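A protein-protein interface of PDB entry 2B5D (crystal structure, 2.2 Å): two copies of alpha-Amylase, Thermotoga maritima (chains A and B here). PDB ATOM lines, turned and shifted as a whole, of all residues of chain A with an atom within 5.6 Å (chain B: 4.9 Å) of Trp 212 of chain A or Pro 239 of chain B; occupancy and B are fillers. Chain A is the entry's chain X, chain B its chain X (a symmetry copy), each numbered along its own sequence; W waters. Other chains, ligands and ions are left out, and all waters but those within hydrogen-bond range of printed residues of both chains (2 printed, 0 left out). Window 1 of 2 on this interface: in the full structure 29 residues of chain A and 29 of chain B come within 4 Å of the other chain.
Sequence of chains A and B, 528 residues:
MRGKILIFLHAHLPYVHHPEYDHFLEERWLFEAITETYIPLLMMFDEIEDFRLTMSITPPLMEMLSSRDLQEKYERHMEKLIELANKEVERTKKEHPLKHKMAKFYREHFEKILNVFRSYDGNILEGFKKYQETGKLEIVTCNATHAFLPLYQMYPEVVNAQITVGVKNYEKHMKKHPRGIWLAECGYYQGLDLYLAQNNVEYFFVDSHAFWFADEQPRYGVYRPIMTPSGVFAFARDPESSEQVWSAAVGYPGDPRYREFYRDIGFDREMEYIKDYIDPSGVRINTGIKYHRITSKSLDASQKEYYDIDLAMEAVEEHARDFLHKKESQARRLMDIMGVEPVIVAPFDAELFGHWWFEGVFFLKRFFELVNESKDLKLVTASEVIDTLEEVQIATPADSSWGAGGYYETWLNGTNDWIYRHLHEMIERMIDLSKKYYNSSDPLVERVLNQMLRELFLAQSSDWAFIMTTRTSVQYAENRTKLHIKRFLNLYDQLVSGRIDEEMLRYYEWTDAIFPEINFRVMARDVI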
ATOM      1  N   SER A 208      10.653  -3.365  14.904  1.00  0.00           N
ATOM      2  CA  SER A 208       9.282  -3.520  14.505  1.00  0.00           C
ATOM      3  C   SER A 208       8.597  -4.641  15.219  1.00  0.00           C
ATOM      4  O   SER A 208       7.415  -4.542  15.528  1.00  0.00           O
ATOM      5  CB  SER A 208       9.246  -3.841  12.973  1.00  0.00           C
ATOM      6  OG  SER A 208       9.773  -2.734  12.299  1.00  0.00           O
ATOM      7  N   HIS A 209       9.330  -5.716  15.471  1.00  0.00           N
ATOM      8  CA  HIS A 209       8.758  -6.869  16.173  1.00  0.00           C
ATOM      9  C   HIS A 209       8.283  -6.519  17.652  1.00  0.00           C
ATOM     10  O   HIS A 209       7.442  -7.234  18.271  1.00  0.00           O
ATOM     11  CB  HIS A 209       9.828  -7.948  16.210  1.00  0.00           C
ATOM     12  CG  HIS A 209       9.360  -9.236  16.788  1.00  0.00           C
ATOM     13  ND1 HIS A 209       9.654  -9.623  18.088  1.00  0.00           N
ATOM     14  CD2 HIS A 209       8.647 -10.250  16.241  1.00  0.00           C
ATOM     15  CE1 HIS A 209       9.121 -10.814  18.316  1.00  0.00           C
ATOM     16  NE2 HIS A 209       8.508 -11.218  17.213  1.00  0.00           N
ATOM     17  N   ALA A 210       8.863  -5.461  18.208  1.00  0.00           N
ATOM     18  CA  ALA A 210       8.471  -5.001  19.542  1.00  0.00           C
ATOM     19  C   ALA A 210       7.013  -4.546  19.575  1.00  0.00           C
ATOM     20  O   ALA A 210       6.359  -4.647  20.629  1.00  0.00           O
ATOM     21  CB  ALA A 210       9.412  -3.851  20.038  1.00  0.00           C
ATOM     22  N   PHE A 211       6.509  -4.021  18.447  1.00  0.00           N
ATOM     23  CA  PHE A 211       5.095  -3.616  18.337  1.00  0.00           C
ATOM     24  C   PHE A 211       4.262  -4.766  17.806  1.00  0.00           C
ATOM     25  O   PHE A 211       3.130  -4.985  18.285  1.00  0.00           O
ATOM     26  CB  PHE A 211       4.895  -2.437  17.410  1.00  0.00           C
ATOM     27  CG  PHE A 211       5.381  -1.084  17.947  1.00  0.00           C
ATOM     28  CD1 PHE A 211       4.877   0.103  17.399  1.00  0.00           C
ATOM     29  CD2 PHE A 211       6.294  -0.992  19.000  1.00  0.00           C
ATOM     30  CE1 PHE A 211       5.312   1.364  17.853  1.00  0.00           C
ATOM     31  CE2 PHE A 211       6.755   0.242  19.453  1.00  0.00           C
ATOM     32  CZ  PHE A 211       6.257   1.432  18.889  1.00  0.00           C
ATOM     33  N   TRP A 212       4.784  -5.492  16.811  1.00  0.00           N
ATOM     34  CA  TRP A 212       3.992  -6.546  16.161  1.00  0.00           C
ATOM     35  C   TRP A 212       3.689  -7.643  17.104  1.00  0.00           C
ATOM     36  O   TRP A 212       2.689  -8.352  16.978  1.00  0.00           O
ATOM     37  CB  TRP A 212       4.706  -7.151  14.926  1.00  0.00           C
ATOM     38  CG  TRP A 212       4.886  -6.159  13.810  1.00  0.00           C
ATOM     39  CD1 TRP A 212       4.099  -5.064  13.544  1.00  0.00           C
ATOM     40  CD2 TRP A 212       5.877  -6.194  12.783  1.00  0.00           C
ATOM     41  NE1 TRP A 212       4.586  -4.383  12.451  1.00  0.00           N
ATOM     42  CE2 TRP A 212       5.669  -5.066  11.959  1.00  0.00           C
ATOM     43  CE3 TRP A 212       6.927  -7.064  12.484  1.00  0.00           C
ATOM     44  CZ2 TRP A 212       6.458  -4.802  10.832  1.00  0.00           C
ATOM     45  CZ3 TRP A 212       7.731  -6.790  11.353  1.00  0.00           C
ATOM     46  CH2 TRP A 212       7.491  -5.665  10.560  1.00  0.00           C
ATOM     47  N   PHE A 213       4.604  -7.863  18.026  1.00  0.00           N
ATOM     48  CA  PHE A 213       4.470  -9.028  18.860  1.00  0.00           C
ATOM     49  C   PHE A 213       4.006  -8.700  20.309  1.00  0.00           C
ATOM     50  O   PHE A 213       3.907  -9.595  21.138  1.00  0.00           O
ATOM     51  CB  PHE A 213       5.761  -9.833  18.809  1.00  0.00           C
ATOM     52  CG  PHE A 213       5.521 -11.289  18.742  1.00  0.00           C
ATOM     53  CD1 PHE A 213       4.981 -11.849  17.598  1.00  0.00           C
ATOM     54  CD2 PHE A 213       5.753 -12.089  19.848  1.00  0.00           C
ATOM     55  CE1 PHE A 213       4.689 -13.207  17.545  1.00  0.00           C
ATOM     56  CE2 PHE A 213       5.503 -13.476  19.807  1.00  0.00           C
ATOM     57  CZ  PHE A 213       4.958 -14.034  18.653  1.00  0.00           C
ATOM     58  N   ALA A 214       3.712  -7.422  20.568  1.00  0.00           N
ATOM     59  CA  ALA A 214       3.051  -6.947  21.781  1.00  0.00           C
ATOM     60  C   ALA A 214       1.683  -7.654  22.031  1.00  0.00           C
ATOM     61  O   ALA A 214       1.066  -8.207  21.097  1.00  0.00           O
ATOM     62  CB  ALA A 214       2.895  -5.451  21.700  1.00  0.00           C
ATOM     63  N   GLN A 217      -1.400  -5.176  19.497  1.00  0.00           N
ATOM     64  CA  GLN A 217      -0.577  -4.395  18.591  1.00  0.00           C
ATOM     65  C   GLN A 217      -1.002  -2.943  18.710  1.00  0.00           C
ATOM     66  O   GLN A 217      -2.181  -2.649  18.778  1.00  0.00           O
ATOM     67  CB  GLN A 217      -0.715  -4.866  17.137  1.00  0.00           C
ATOM     68  CG  GLN A 217      -0.126  -6.248  16.817  1.00  0.00           C
ATOM     69  CD  GLN A 217       0.043  -6.470  15.297  1.00  0.00           C
ATOM     70  OE1 GLN A 217       0.770  -7.378  14.837  1.00  0.00           O
ATOM     71  NE2 GLN A 217      -0.657  -5.652  14.513  1.00  0.00           N
ATOM     72  N   PRO A 218      -0.039  -2.024  18.789  1.00  0.00           N
ATOM     73  CA  PRO A 218      -0.338  -0.592  18.622  1.00  0.00           C
ATOM     74  C   PRO A 218      -1.225  -0.251  17.416  1.00  0.00           C
ATOM     75  O   PRO A 218      -0.992  -0.740  16.306  1.00  0.00           O
ATOM     76  CB  PRO A 218       1.037   0.013  18.454  1.00  0.00           C
ATOM     77  CG  PRO A 218       1.920  -0.880  19.318  1.00  0.00           C
ATOM     78  CD  PRO A 218       1.367  -2.269  19.136  1.00  0.00           C
ATOM     79  N   VAL A 222       3.785   0.840  13.331  1.00  0.00           N
ATOM     80  CA  VAL A 222       5.083   1.426  13.637  1.00  0.00           C
ATOM     81  C   VAL A 222       5.170   2.874  13.318  1.00  0.00           C
ATOM     82  O   VAL A 222       6.224   3.485  13.483  1.00  0.00           O
ATOM     83  CB  VAL A 222       6.266   0.688  12.952  1.00  0.00           C
ATOM     84  CG1 VAL A 222       6.337  -0.714  13.460  1.00  0.00           C
ATOM     85  CG2 VAL A 222       6.158   0.720  11.350  1.00  0.00           C
ATOM     86  N   PRO A 239       9.904  -0.852   8.734  1.00  0.00           N
ATOM     87  CA  PRO A 239      10.584  -1.950   8.070  1.00  0.00           C
ATOM     88  C   PRO A 239      10.624  -1.767   6.515  1.00  0.00           C
ATOM     89  O   PRO A 239      11.369  -2.470   5.837  1.00  0.00           O
ATOM     90  CB  PRO A 239       9.706  -3.164   8.421  1.00  0.00           C
ATOM     91  CG  PRO A 239       8.284  -2.532   8.676  1.00  0.00           C
ATOM     92  CD  PRO A 239       8.515  -1.170   9.143  1.00  0.00           C
ATOM     93  N   SER B 208       9.855  -9.436   1.863  1.00  0.00           N
ATOM     94  CA  SER B 208       8.919  -8.352   1.972  1.00  0.00           C
ATOM     95  C   SER B 208       9.361  -7.132   1.226  1.00  0.00           C
ATOM     96  O   SER B 208       8.535  -6.423   0.664  1.00  0.00           O
ATOM     97  CB  SER B 208       8.785  -7.962   3.482  1.00  0.00           C
ATOM     98  OG  SER B 208       8.251  -9.067   4.155  1.00  0.00           O
ATOM     99  N   TRP B 212       7.625  -4.046  -1.067  1.00  0.00           N
ATOM    100  CA  TRP B 212       7.654  -2.684  -0.513  1.00  0.00           C
ATOM    101  C   TRP B 212       8.395  -1.764  -1.401  1.00  0.00           C
ATOM    102  O   TRP B 212       8.155  -0.556  -1.431  1.00  0.00           O
ATOM    103  CB  TRP B 212       8.301  -2.628   0.893  1.00  0.00           C
ATOM    104  CG  TRP B 212       7.508  -3.374   1.933  1.00  0.00           C
ATOM    105  CD1 TRP B 212       6.154  -3.605   1.928  1.00  0.00           C
ATOM    106  CD2 TRP B 212       8.003  -3.937   3.147  1.00  0.00           C
ATOM    107  NE1 TRP B 212       5.794  -4.337   3.037  1.00  0.00           N
ATOM    108  CE2 TRP B 212       6.911  -4.541   3.807  1.00  0.00           C
ATOM    109  CE3 TRP B 212       9.267  -3.999   3.739  1.00  0.00           C
ATOM    110  CZ2 TRP B 212       7.039  -5.174   5.050  1.00  0.00           C
ATOM    111  CZ3 TRP B 212       9.397  -4.650   4.988  1.00  0.00           C
ATOM    112  CH2 TRP B 212       8.291  -5.232   5.610  1.00  0.00           C
ATOM    113  N   VAL B 222       1.852  -7.650   1.557  1.00  0.00           N
ATOM    114  CA  VAL B 222       2.422  -8.989   1.488  1.00  0.00           C
ATOM    115  C   VAL B 222       1.424 -10.070   1.692  1.00  0.00           C
ATOM    116  O   VAL B 222       1.777 -11.247   1.705  1.00  0.00           O
ATOM    117  CB  VAL B 222       3.605  -9.204   2.472  1.00  0.00           C
ATOM    118  CG1 VAL B 222       4.722  -8.281   2.114  1.00  0.00           C
ATOM    119  CG2 VAL B 222       3.164  -9.014   4.004  1.00  0.00           C
ATOM    120  N   TYR B 223       0.160  -9.679   1.841  1.00  0.00           N
ATOM    121  CA  TYR B 223      -0.931 -10.617   2.203  1.00  0.00           C
ATOM    122  C   TYR B 223      -1.772 -11.127   1.036  1.00  0.00           C
ATOM    123  O   TYR B 223      -2.790 -11.791   1.231  1.00  0.00           O
ATOM    124  CB  TYR B 223      -1.851  -9.977   3.298  1.00  0.00           C
ATOM    125  CG  TYR B 223      -0.990  -9.597   4.474  1.00  0.00           C
ATOM    126  CD1 TYR B 223      -0.415 -10.588   5.274  1.00  0.00           C
ATOM    127  CD2 TYR B 223      -0.693  -8.254   4.738  1.00  0.00           C
ATOM    128  CE1 TYR B 223       0.422 -10.248   6.363  1.00  0.00           C
ATOM    129  CE2 TYR B 223       0.109  -7.911   5.808  1.00  0.00           C
ATOM    130  CZ  TYR B 223       0.672  -8.906   6.602  1.00  0.00           C
ATOM    131  OH  TYR B 223       1.529  -8.557   7.610  1.00  0.00           O
ATOM    132  N   ARG B 237       6.987 -12.930   2.110  1.00  0.00           N
ATOM    133  CA  ARG B 237       7.129 -13.119   3.582  1.00  0.00           C
ATOM    134  C   ARG B 237       6.276 -12.145   4.409  1.00  0.00           C
ATOM    135  O   ARG B 237       6.412 -10.928   4.247  1.00  0.00           O
ATOM    136  CB  ARG B 237       8.598 -12.829   3.937  1.00  0.00           C
ATOM    137  CG  ARG B 237       9.216 -13.802   4.791  1.00  0.00           C
ATOM    138  CD  ARG B 237      10.611 -13.369   5.072  1.00  0.00           C
ATOM    139  NE  ARG B 237      10.692 -12.395   6.165  1.00  0.00           N
ATOM    140  CZ  ARG B 237      11.079 -11.159   5.947  1.00  0.00           C
ATOM    141  NH1 ARG B 237      11.146 -10.248   6.908  1.00  0.00           N
ATOM    142  NH2 ARG B 237      11.382 -10.853   4.697  1.00  0.00           N
ATOM    143  N   ASP B 238       5.487 -12.674   5.336  1.00  0.00           N
ATOM    144  CA  ASP B 238       4.843 -11.825   6.390  1.00  0.00           C
ATOM    145  C   ASP B 238       5.903 -11.477   7.423  1.00  0.00           C
ATOM    146  O   ASP B 238       6.372 -12.349   8.144  1.00  0.00           O
ATOM    147  CB  ASP B 238       3.656 -12.566   7.065  1.00  0.00           C
ATOM    148  CG  ASP B 238       3.109 -11.827   8.312  1.00  0.00           C
ATOM    149  OD1 ASP B 238       3.305 -10.591   8.502  1.00  0.00           O
ATOM    150  OD2 ASP B 238       2.460 -12.518   9.094  1.00  0.00           O
ATOM    151  N   PRO B 239       6.291 -10.211   7.489  1.00  0.00           N
ATOM    152  CA  PRO B 239       7.374  -9.824   8.376  1.00  0.00           C
ATOM    153  C   PRO B 239       6.943  -9.850   9.881  1.00  0.00           C
ATOM    154  O   PRO B 239       7.798  -9.791  10.761  1.00  0.00           O
ATOM    155  CB  PRO B 239       7.666  -8.374   7.950  1.00  0.00           C
ATOM    156  CG  PRO B 239       6.297  -7.882   7.342  1.00  0.00           C
ATOM    157  CD  PRO B 239       5.627  -9.067   6.820  1.00  0.00           C
ATOM    158  N   GLU B 240       5.639  -9.891  10.139  1.00  0.00           N
ATOM    159  CA  GLU B 240       5.087 -10.106  11.464  1.00  0.00           C
ATOM    160  C   GLU B 240       5.260 -11.542  11.896  1.00  0.00           C
ATOM    161  O   GLU B 240       5.220 -11.818  13.106  1.00  0.00           O
ATOM    162  CB  GLU B 240       3.602  -9.742  11.523  1.00  0.00           C
ATOM    163  CG  GLU B 240       3.348  -8.308  11.264  1.00  0.00           C
ATOM    164  CD  GLU B 240       1.942  -7.893  11.666  1.00  0.00           C
ATOM    165  OE1 GLU B 240       1.543  -6.762  11.318  1.00  0.00           O
ATOM    166  OE2 GLU B 240       1.237  -8.682  12.325  1.00  0.00           O
ATOM    167  N   SER B 241       5.439 -12.460  10.942  1.00  0.00           N
ATOM    168  CA  SER B 241       5.784 -13.829  11.305  1.00  0.00           C
ATOM    169  C   SER B 241       7.308 -14.115  11.111  1.00  0.00           C
ATOM    170  O   SER B 241       7.694 -15.194  10.724  1.00  0.00           O
ATOM    171  CB  SER B 241       4.914 -14.846  10.573  1.00  0.00           C
ATOM    172  OG  SER B 241       3.515 -14.549  10.592  1.00  0.00           O
ATOM    173  N   SER B 242       8.174 -13.136  11.383  1.00  0.00           N
ATOM    174  CA  SER B 242       9.634 -13.275  11.194  1.00  0.00           C
ATOM    175  C   SER B 242      10.350 -14.288  12.094  1.00  0.00           C
ATOM    176  O   SER B 242       9.764 -14.854  13.017  1.00  0.00           O
ATOM    177  CB  SER B 242      10.334 -11.926  11.412  1.00  0.00           C
ATOM    178  OG  SER B 242      10.676 -11.750  12.812  1.00  0.00           O
HETATM  179  O   HOH W   1       0.105  -4.920  12.055  1.00  0.00           O
HETATM  180  O   HOH W   2       1.050 -10.537  13.902  1.00  0.00           O
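The side-chain amide oxygen (OE1) of Gln 217 of chain A lies close to the side-chain carboxylate (OE2) of Glu 240 of chain B, at 2.9 Å.
The side-chain amide oxygen of Gln 217 of chain A lies close to the backbone carbonyl oxygen of Trp 212 of chain A (3.0 Å).
OD1 of Asp 238 of chain B lies within hydrogen-bond range of N of Glu 240 of chain B (2.9 Å).
O of Pro 239 of chain B touches CZ3 of Trp 212 of chain A (3.1 Å).
Trp 212 of chain A touches Glu 240 of chain B.
Pro 239 of chain A touches Trp 212 of chain B.
His 209 of chain A touches none of the printed residues of chain B.
Of chain B, only Pro 239 (3.1 Å) and Glu 240 (3.6 Å) come within 4 Å of Trp 212 of chain A.
Of the printed residues of chain B, Gln 217 of chain A touches Glu 240 (2.9 Å).
Of the printed residues of chain B, Pro 239 of chain A touches Trp 212 (3.1 Å).
Of the printed residues of chain A, Trp 212 of chain B touches Pro 239.
Of chain A, only Trp 212 comes within 4 Å of Pro 239 of chain B.
Printed residues of chain A within 4 Å of Glu 240 of chain B: Trp 212 (3.6 Å) and Gln 217 (2.9 Å).
The nearest printed residue of chain B that does not touch Trp 212 of chain A is Trp 212 of chain B (5.0 Å).
The nearest printed residue of chain B that does not touch Pro 239 of chain A is Pro 239 of chain B (5.6 Å).
Printed residues of chain A that touch a printed residue of chain B: Trp 212, Gln 217 and Pro 239.
Hydrophobic or aromatic side chains of chain A within 4 Å of the printed part of chain B: Trp 212 and Pro 239.
Of the 10 printed residues of chain B, 3 touch a printed residue of chain A.
Among the printed residues, no Asp or Glu carboxylate lies within 4 Å of a Lys or Arg side-chain nitrogen of the other chain.
Trp 212 of chain A touches Pro 239 of chain B, and with the chains exchanged Pro 239 of chain A touches Trp 212 of chain B.
Of the 4 pairs that touch across the chains among the printed residues, 2 have their exchanged pair printed and touching as well.
Water W2 bridges the side-chain carboxylate (OE2) of Glu 240 of chain B (2.4 Å) and the side-chain amide oxygen (OE1) of Gln 217 of chain A (3.3 Å).
Water W1 lies within hydrogen-bond range of the side-chain carboxylate of Glu 240 of chain B (2.5 Å) and the side-chain amide nitrogen of Gln 217 of chain A (2.7 Å).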
